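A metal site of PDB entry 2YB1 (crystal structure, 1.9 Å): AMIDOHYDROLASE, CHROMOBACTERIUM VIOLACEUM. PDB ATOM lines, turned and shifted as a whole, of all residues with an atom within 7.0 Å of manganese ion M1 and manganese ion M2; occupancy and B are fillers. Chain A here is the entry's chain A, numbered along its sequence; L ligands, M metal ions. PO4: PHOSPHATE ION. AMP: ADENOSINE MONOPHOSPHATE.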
ATOM      1  N   HIS A   7     -16.138 -26.531  13.899  1.00  0.00           N
ATOM      2  CA  HIS A   7     -16.678 -26.485  15.259  1.00  0.00           C
ATOM      3  C   HIS A   7     -16.898 -25.053  15.782  1.00  0.00           C
ATOM      4  O   HIS A   7     -15.936 -24.323  15.953  1.00  0.00           O
ATOM      5  CB  HIS A   7     -15.690 -27.229  16.174  1.00  0.00           C
ATOM      6  CG  HIS A   7     -16.200 -27.505  17.555  1.00  0.00           C
ATOM      7  ND1 HIS A   7     -15.854 -28.640  18.257  1.00  0.00           N
ATOM      8  CD2 HIS A   7     -16.995 -26.776  18.375  1.00  0.00           C
ATOM      9  CE1 HIS A   7     -16.425 -28.612  19.440  1.00  0.00           C
ATOM     10  NE2 HIS A   7     -17.120 -27.497  19.542  1.00  0.00           N
ATOM     11  N   PHE A   8     -18.135 -24.674  16.072  1.00  0.00           N
ATOM     12  CA  PHE A   8     -18.422 -23.392  16.735  1.00  0.00           C
ATOM     13  C   PHE A   8     -19.874 -23.345  17.198  1.00  0.00           C
ATOM     14  O   PHE A   8     -20.669 -24.220  16.833  1.00  0.00           O
ATOM     15  CB  PHE A   8     -18.072 -22.176  15.825  1.00  0.00           C
ATOM     16  CG  PHE A   8     -18.688 -22.222  14.434  1.00  0.00           C
ATOM     17  CD1 PHE A   8     -19.948 -21.669  14.183  1.00  0.00           C
ATOM     18  CD2 PHE A   8     -17.965 -22.747  13.356  1.00  0.00           C
ATOM     19  CE1 PHE A   8     -20.506 -21.702  12.897  1.00  0.00           C
ATOM     20  CE2 PHE A   8     -18.517 -22.788  12.069  1.00  0.00           C
ATOM     21  CZ  PHE A   8     -19.796 -22.254  11.841  1.00  0.00           C
ATOM     22  N   HIS A   9     -20.221 -22.302  17.944  1.00  0.00           N
ATOM     23  CA  HIS A   9     -21.496 -22.223  18.649  1.00  0.00           C
ATOM     24  C   HIS A   9     -22.265 -20.947  18.357  1.00  0.00           C
ATOM     25  O   HIS A   9     -21.692 -19.963  17.886  1.00  0.00           O
ATOM     26  CB  HIS A   9     -21.278 -22.335  20.164  1.00  0.00           C
ATOM     27  CG  HIS A   9     -20.713 -23.658  20.562  1.00  0.00           C
ATOM     28  ND1 HIS A   9     -21.515 -24.705  20.975  1.00  0.00           N
ATOM     29  CD2 HIS A   9     -19.452 -24.129  20.554  1.00  0.00           C
ATOM     30  CE1 HIS A   9     -20.754 -25.752  21.224  1.00  0.00           C
ATOM     31  NE2 HIS A   9     -19.505 -25.432  20.978  1.00  0.00           N
ATOM     32  N   ASP A  14     -24.688 -22.272  23.677  1.00  0.00           N
ATOM     33  CA  ASP A  14     -23.844 -21.385  24.491  1.00  0.00           C
ATOM     34  C   ASP A  14     -23.004 -20.300  23.801  1.00  0.00           C
ATOM     35  O   ASP A  14     -22.160 -19.675  24.440  1.00  0.00           O
ATOM     36  CB  ASP A  14     -23.076 -22.138  25.593  1.00  0.00           C
ATOM     37  CG  ASP A  14     -21.971 -22.978  25.036  1.00  0.00           C
ATOM     38  OD1 ASP A  14     -21.905 -23.128  23.803  1.00  0.00           O
ATOM     39  OD2 ASP A  14     -21.170 -23.479  25.845  1.00  0.00           O
ATOM     40  N   THR A  37     -21.912 -26.333  15.237  1.00  0.00           N
ATOM     41  CA  THR A  37     -22.152 -27.483  16.095  1.00  0.00           C
ATOM     42  C   THR A  37     -22.545 -27.013  17.485  1.00  0.00           C
ATOM     43  O   THR A  37     -21.719 -26.994  18.407  1.00  0.00           O
ATOM     44  CB  THR A  37     -20.825 -28.278  16.197  1.00  0.00           C
ATOM     45  OG1 THR A  37     -19.791 -27.419  16.684  1.00  0.00           O
ATOM     46  CG2 THR A  37     -20.389 -28.744  14.824  1.00  0.00           C
ATOM     47  N   ASP A  38     -23.839 -26.813  17.677  1.00  0.00           N
ATOM     48  CA  ASP A  38     -24.348 -26.390  18.976  1.00  0.00           C
ATOM     49  C   ASP A  38     -24.486 -27.596  19.875  1.00  0.00           C
ATOM     50  O   ASP A  38     -24.658 -28.724  19.390  1.00  0.00           O
ATOM     51  CB  ASP A  38     -25.671 -25.647  18.820  1.00  0.00           C
ATOM     52  CG  ASP A  38     -25.462 -24.178  18.493  1.00  0.00           C
ATOM     53  OD1 ASP A  38     -24.770 -23.488  19.264  1.00  0.00           O
ATOM     54  OD2 ASP A  38     -25.991 -23.723  17.457  1.00  0.00           O
ATOM     55  N   HIS A  39     -24.399 -27.355  21.184  1.00  0.00           N
ATOM     56  CA  HIS A  39     -24.531 -28.431  22.171  1.00  0.00           C
ATOM     57  C   HIS A  39     -25.920 -29.044  22.162  1.00  0.00           C
ATOM     58  O   HIS A  39     -26.908 -28.326  22.316  1.00  0.00           O
ATOM     59  CB  HIS A  39     -24.292 -27.875  23.576  1.00  0.00           C
ATOM     60  CG  HIS A  39     -22.892 -27.409  23.829  1.00  0.00           C
ATOM     61  ND1 HIS A  39     -21.844 -28.287  23.995  1.00  0.00           N
ATOM     62  CD2 HIS A  39     -22.384 -26.173  23.981  1.00  0.00           C
ATOM     63  CE1 HIS A  39     -20.737 -27.598  24.238  1.00  0.00           C
ATOM     64  NE2 HIS A  39     -21.034 -26.315  24.231  1.00  0.00           N
ATOM     65  N   GLU A  64     -22.908 -30.847  18.668  1.00  0.00           N
ATOM     66  CA  GLU A  64     -21.957 -31.340  19.656  1.00  0.00           C
ATOM     67  C   GLU A  64     -22.695 -32.041  20.798  1.00  0.00           C
ATOM     68  O   GLU A  64     -23.430 -31.400  21.582  1.00  0.00           O
ATOM     69  CB  GLU A  64     -21.083 -30.196  20.209  1.00  0.00           C
ATOM     70  CG  GLU A  64     -20.037 -30.729  21.189  1.00  0.00           C
ATOM     71  CD  GLU A  64     -19.056 -29.688  21.634  1.00  0.00           C
ATOM     72  OE1 GLU A  64     -19.384 -28.494  21.568  1.00  0.00           O
ATOM     73  OE2 GLU A  64     -17.948 -30.077  22.035  1.00  0.00           O
ATOM     74  N   VAL A  74     -17.277 -36.343  27.997  1.00  0.00           N
ATOM     75  CA  VAL A  74     -16.643 -36.089  26.710  1.00  0.00           C
ATOM     76  C   VAL A  74     -17.667 -35.504  25.747  1.00  0.00           C
ATOM     77  O   VAL A  74     -18.879 -35.615  25.971  1.00  0.00           O
ATOM     78  CB  VAL A  74     -15.977 -37.356  26.093  1.00  0.00           C
ATOM     79  CG1 VAL A  74     -14.842 -37.872  26.995  1.00  0.00           C
ATOM     80  CG2 VAL A  74     -16.996 -38.432  25.841  1.00  0.00           C
ATOM     81  N   HIS A  75     -17.182 -34.845  24.696  1.00  0.00           N
ATOM     82  CA  HIS A  75     -18.067 -34.262  23.699  1.00  0.00           C
ATOM     83  C   HIS A  75     -17.829 -34.881  22.331  1.00  0.00           C
ATOM     84  O   HIS A  75     -16.685 -34.959  21.870  1.00  0.00           O
ATOM     85  CB  HIS A  75     -17.881 -32.742  23.643  1.00  0.00           C
ATOM     86  CG  HIS A  75     -18.445 -32.025  24.826  1.00  0.00           C
ATOM     87  ND1 HIS A  75     -18.179 -30.702  25.104  1.00  0.00           N
ATOM     88  CD2 HIS A  75     -19.281 -32.445  25.811  1.00  0.00           C
ATOM     89  CE1 HIS A  75     -18.821 -30.333  26.193  1.00  0.00           C
ATOM     90  NE2 HIS A  75     -19.509 -31.374  26.634  1.00  0.00           N
ATOM     91  N   ILE A  76     -18.910 -35.360  21.711  1.00  0.00           N
ATOM     92  CA  ILE A  76     -18.823 -35.986  20.394  1.00  0.00           C
ATOM     93  C   ILE A  76     -19.559 -35.122  19.378  1.00  0.00           C
ATOM     94  O   ILE A  76     -20.782 -34.940  19.470  1.00  0.00           O
ATOM     95  CB  ILE A  76     -19.451 -37.427  20.389  1.00  0.00           C
ATOM     96  CG1 ILE A  76     -18.786 -38.303  21.455  1.00  0.00           C
ATOM     97  CG2 ILE A  76     -19.378 -38.053  18.998  1.00  0.00           C
ATOM     98  CD1 ILE A  76     -17.273 -38.487  21.255  1.00  0.00           C
ATOM     99  N   VAL A  77     -18.821 -34.578  18.424  1.00  0.00           N
ATOM    100  CA  VAL A  77     -19.390 -33.791  17.337  1.00  0.00           C
ATOM    101  C   VAL A  77     -19.975 -34.702  16.249  1.00  0.00           C
ATOM    102  O   VAL A  77     -19.377 -35.739  15.925  1.00  0.00           O
ATOM    103  CB  VAL A  77     -18.303 -32.873  16.719  1.00  0.00           C
ATOM    104  CG1 VAL A  77     -18.687 -32.446  15.299  1.00  0.00           C
ATOM    105  CG2 VAL A  77     -18.054 -31.655  17.625  1.00  0.00           C
ATOM    106  N   ALA A 190     -14.393 -34.606  20.103  1.00  0.00           N
ATOM    107  CA  ALA A 190     -14.080 -33.189  20.110  1.00  0.00           C
ATOM    108  C   ALA A 190     -12.951 -32.875  21.100  1.00  0.00           C
ATOM    109  O   ALA A 190     -12.843 -33.522  22.131  1.00  0.00           O
ATOM    110  CB  ALA A 190     -15.327 -32.368  20.445  1.00  0.00           C
ATOM    111  N   HIS A 191     -12.104 -31.925  20.719  1.00  0.00           N
ATOM    112  CA  HIS A 191     -11.083 -31.359  21.606  1.00  0.00           C
ATOM    113  C   HIS A 191     -10.520 -32.345  22.639  1.00  0.00           C
ATOM    114  O   HIS A 191     -10.599 -32.123  23.837  1.00  0.00           O
ATOM    115  CB  HIS A 191     -11.590 -30.056  22.276  1.00  0.00           C
ATOM    116  CG  HIS A 191     -12.879 -30.223  23.017  1.00  0.00           C
ATOM    117  ND1 HIS A 191     -13.017 -31.077  24.084  1.00  0.00           N
ATOM    118  CD2 HIS A 191     -14.088 -29.620  22.849  1.00  0.00           C
ATOM    119  CE1 HIS A 191     -14.256 -31.006  24.541  1.00  0.00           C
ATOM    120  NE2 HIS A 191     -14.915 -30.131  23.810  1.00  0.00           N
ATOM    121  N   ARG A 194      -8.403 -31.613  25.944  1.00  0.00           N
ATOM    122  CA  ARG A 194      -9.033 -31.063  27.146  1.00  0.00           C
ATOM    123  C   ARG A 194      -9.341 -32.133  28.194  1.00  0.00           C
ATOM    124  O   ARG A 194      -9.588 -31.817  29.353  1.00  0.00           O
ATOM    125  CB  ARG A 194     -10.332 -30.311  26.817  1.00  0.00           C
ATOM    126  CG  ARG A 194     -10.163 -29.067  25.975  1.00  0.00           C
ATOM    127  CD  ARG A 194     -10.823 -27.855  26.651  1.00  0.00           C
ATOM    128  NE  ARG A 194     -12.178 -28.121  27.148  1.00  0.00           N
ATOM    129  CZ  ARG A 194     -13.295 -27.592  26.627  1.00  0.00           C
ATOM    130  NH1 ARG A 194     -13.224 -26.780  25.582  1.00  0.00           N
ATOM    131  NH2 ARG A 194     -14.479 -27.885  27.161  1.00  0.00           N
ATOM    132  N   TYR A 195      -9.350 -33.403  27.787  1.00  0.00           N
ATOM    133  CA  TYR A 195      -9.801 -34.456  28.695  1.00  0.00           C
ATOM    134  C   TYR A 195      -8.687 -34.835  29.674  1.00  0.00           C
ATOM    135  O   TYR A 195      -7.496 -34.794  29.314  1.00  0.00           O
ATOM    136  CB  TYR A 195     -10.264 -35.678  27.906  1.00  0.00           C
ATOM    137  CG  TYR A 195     -11.359 -35.379  26.887  1.00  0.00           C
ATOM    138  CD1 TYR A 195     -12.375 -34.489  27.178  1.00  0.00           C
ATOM    139  CD2 TYR A 195     -11.364 -35.999  25.643  1.00  0.00           C
ATOM    140  CE1 TYR A 195     -13.374 -34.208  26.251  1.00  0.00           C
ATOM    141  CE2 TYR A 195     -12.359 -35.739  24.711  1.00  0.00           C
ATOM    142  CZ  TYR A 195     -13.361 -34.843  25.026  1.00  0.00           C
ATOM    143  OH  TYR A 195     -14.360 -34.551  24.113  1.00  0.00           O
ATOM    144  N   GLU A 218     -10.915 -34.486  16.491  1.00  0.00           N
ATOM    145  CA  GLU A 218     -10.398 -33.142  16.266  1.00  0.00           C
ATOM    146  C   GLU A 218      -8.908 -33.128  16.524  1.00  0.00           C
ATOM    147  O   GLU A 218      -8.429 -33.522  17.580  1.00  0.00           O
ATOM    148  CB  GLU A 218     -11.128 -32.120  17.143  1.00  0.00           C
ATOM    149  CG  GLU A 218     -12.536 -31.854  16.648  1.00  0.00           C
ATOM    150  CD  GLU A 218     -13.285 -30.810  17.455  1.00  0.00           C
ATOM    151  OE1 GLU A 218     -12.815 -30.418  18.544  1.00  0.00           O
ATOM    152  OE2 GLU A 218     -14.370 -30.404  16.989  1.00  0.00           O
ATOM    153  N   SER A 223      -8.948 -25.284  21.165  1.00  0.00           N
ATOM    154  CA  SER A 223      -8.571 -25.753  22.500  1.00  0.00           C
ATOM    155  C   SER A 223      -7.232 -26.504  22.551  1.00  0.00           C
ATOM    156  O   SER A 223      -6.851 -27.011  23.605  1.00  0.00           O
ATOM    157  CB  SER A 223      -9.661 -26.668  23.087  1.00  0.00           C
ATOM    158  OG  SER A 223     -10.925 -26.007  23.157  1.00  0.00           O
ATOM    159  N   ASP A 248     -13.926 -23.862  17.803  1.00  0.00           N
ATOM    160  CA  ASP A 248     -14.716 -23.919  19.027  1.00  0.00           C
ATOM    161  C   ASP A 248     -15.066 -22.516  19.505  1.00  0.00           C
ATOM    162  O   ASP A 248     -15.183 -22.260  20.707  1.00  0.00           O
ATOM    163  CB  ASP A 248     -13.972 -24.681  20.145  1.00  0.00           C
ATOM    164  CG  ASP A 248     -14.897 -25.080  21.280  1.00  0.00           C
ATOM    165  OD1 ASP A 248     -16.137 -25.116  21.081  1.00  0.00           O
ATOM    166  OD2 ASP A 248     -14.390 -25.360  22.391  1.00  0.00           O
ATOM    167  N   PHE A 249     -15.276 -21.616  18.550  1.00  0.00           N
ATOM    168  CA  PHE A 249     -15.672 -20.243  18.846  1.00  0.00           C
ATOM    169  C   PHE A 249     -17.001 -20.162  19.596  1.00  0.00           C
ATOM    170  O   PHE A 249     -17.967 -20.841  19.251  1.00  0.00           O
ATOM    171  CB  PHE A 249     -15.751 -19.438  17.538  1.00  0.00           C
ATOM    172  CG  PHE A 249     -16.223 -18.017  17.732  1.00  0.00           C
ATOM    173  CD1 PHE A 249     -17.578 -17.709  17.683  1.00  0.00           C
ATOM    174  CD2 PHE A 249     -15.306 -17.002  17.963  1.00  0.00           C
ATOM    175  CE1 PHE A 249     -18.021 -16.416  17.868  1.00  0.00           C
ATOM    176  CE2 PHE A 249     -15.733 -15.708  18.140  1.00  0.00           C
ATOM    177  CZ  PHE A 249     -17.089 -15.403  18.101  1.00  0.00           C
ATOM    178  N   HIS A 250     -17.036 -19.324  20.643  1.00  0.00           N
ATOM    179  CA  HIS A 250     -18.244 -19.018  21.429  1.00  0.00           C
ATOM    180  C   HIS A 250     -18.566 -17.538  21.346  1.00  0.00           C
ATOM    181  O   HIS A 250     -19.701 -17.153  21.077  1.00  0.00           O
ATOM    182  CB  HIS A 250     -18.105 -19.413  22.908  1.00  0.00           C
ATOM    183  CG  HIS A 250     -18.191 -20.877  23.159  1.00  0.00           C
ATOM    184  ND1 HIS A 250     -17.208 -21.761  22.761  1.00  0.00           N
ATOM    185  CD2 HIS A 250     -19.134 -21.623  23.781  1.00  0.00           C
ATOM    186  CE1 HIS A 250     -17.538 -22.987  23.127  1.00  0.00           C
ATOM    187  NE2 HIS A 250     -18.708 -22.928  23.747  1.00  0.00           N
HETATM  188  P   PO4 L   1     -16.946 -26.731  24.181  1.00  0.00           P
HETATM  189  O1  PO4 L   1     -15.801 -25.862  24.655  1.00  0.00           O
HETATM  190  O2  PO4 L   1     -18.107 -25.856  23.822  1.00  0.00           O
HETATM  191  O3  PO4 L   1     -16.552 -27.504  22.940  1.00  0.00           O
HETATM  192  O4  PO4 L   1     -17.307 -27.697  25.282  1.00  0.00           O
HETATM  193  P   AMP L   2     -22.498 -27.715  30.507  1.00  0.00           P
HETATM  194  O1P AMP L   2     -21.737 -28.569  31.497  1.00  0.00           O
HETATM  195  O2P AMP L   2     -22.732 -28.547  29.258  1.00  0.00           O
HETATM  196  O3P AMP L   2     -23.701 -27.096  31.179  1.00  0.00           O
HETATM  197  O5' AMP L   2     -21.425 -26.580  30.196  1.00  0.00           O
HETATM  198  C5' AMP L   2     -20.204 -26.900  29.555  1.00  0.00           C
HETATM  199  C4' AMP L   2     -19.664 -25.725  28.775  1.00  0.00           C
HETATM  200  O4' AMP L   2     -18.986 -24.827  29.684  1.00  0.00           O
HETATM  201  C3' AMP L   2     -18.612 -26.067  27.728  1.00  0.00           C
HETATM  202  O3' AMP L   2     -19.176 -26.496  26.502  1.00  0.00           O
HETATM  203  C2' AMP L   2     -17.802 -24.771  27.603  1.00  0.00           C
HETATM  204  O2' AMP L   2     -18.457 -23.868  26.724  1.00  0.00           O
HETATM  205  C1' AMP L   2     -17.889 -24.212  29.027  1.00  0.00           C
HETATM  206  N9  AMP L   2     -16.660 -24.495  29.797  1.00  0.00           N
HETATM  207  C8  AMP L   2     -16.399 -25.618  30.500  1.00  0.00           C
HETATM  208  N7  AMP L   2     -15.166 -25.548  31.073  1.00  0.00           N
HETATM  209  C5  AMP L   2     -14.627 -24.357  30.726  1.00  0.00           C
HETATM  210  C6  AMP L   2     -13.364 -23.629  30.989  1.00  0.00           C
HETATM  211  N6  AMP L   2     -12.388 -24.180  31.756  1.00  0.00           N
HETATM  212  N1  AMP L   2     -13.205 -22.402  30.444  1.00  0.00           N
HETATM  213  C2  AMP L   2     -14.163 -21.837  29.672  1.00  0.00           C
HETATM  214  N3  AMP L   2     -15.338 -22.432  29.394  1.00  0.00           N
HETATM  215  C4  AMP L   2     -15.617 -23.665  29.891  1.00  0.00           C
HETATM  216 MN    MN M   1     -16.938 -29.420  23.770  1.00  0.00          MN
HETATM  217 MN    MN M   2     -17.896 -26.787  21.468  1.00  0.00          MN
HETATM  218 MN    MN M   3     -19.667 -24.690  24.834  1.00  0.00          MN
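The backbone carbonyl oxygen of Asp 38 sits at hydrogen-bond distance from the backbone NH of Glu 64, at 2.8 Å. The backbone NH (N) of His 191 lies within hydrogen-bond range of the side-chain carboxylate (OE1) of Glu 218 (2.7 Å). The backbone carbonyl oxygen (O) of Thr 37 sits close to a ring nitrogen (ND1) of His 9. ND1 of His 9 is in hydrogen-bond range of OD1 of Asp 14. The side-chain carboxylate (OE2) of Glu 218 sits at hydrogen-bond distance from a ring nitrogen (ND1) of His 7. O of His 75 lies within hydrogen-bond range of N of Ala 190, at 2.9 Å. O of Asp 248 is in hydrogen-bond range of ND1 of His 250, 2.9 Å away. The guanidinium group (NH1) of Arg 194 lies within salt-bridge range of the side-chain carboxylate (OD2) of Asp 248.
Three residues have an atom within 4 Å of manganese ion M1: Glu 64, His 75 and His 191. The nearest printed residue that does not touch manganese ion M1 is His 39 (4.2 Å).
Within 4 Å of manganese ion M2: His 7, His 9, Glu 64 and Asp 248.
Manganese ion M1 is bound by the side-chain carboxylate of Glu 64 (2.1 Å), an oxygen (O3) of PO4 L1 (2.1 Å), a ring nitrogen (NE2) of His 191 (2.1 Å), a ring nitrogen (ND1) of His 75 (2.2 Å) and an oxygen (O4) of PO4 L1 (2.3 Å). Manganese ion M1 has five donor atoms within binding distance.
Manganese ion M2 is bound by an oxygen (O3) of PO4 L1, a ring nitrogen (NE2) of His 9, a ring nitrogen (NE2) of His 7, the side-chain carboxylate of Glu 64, the side-chain carboxylate of Asp 248 and an oxygen (O2) of PO4 L1.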
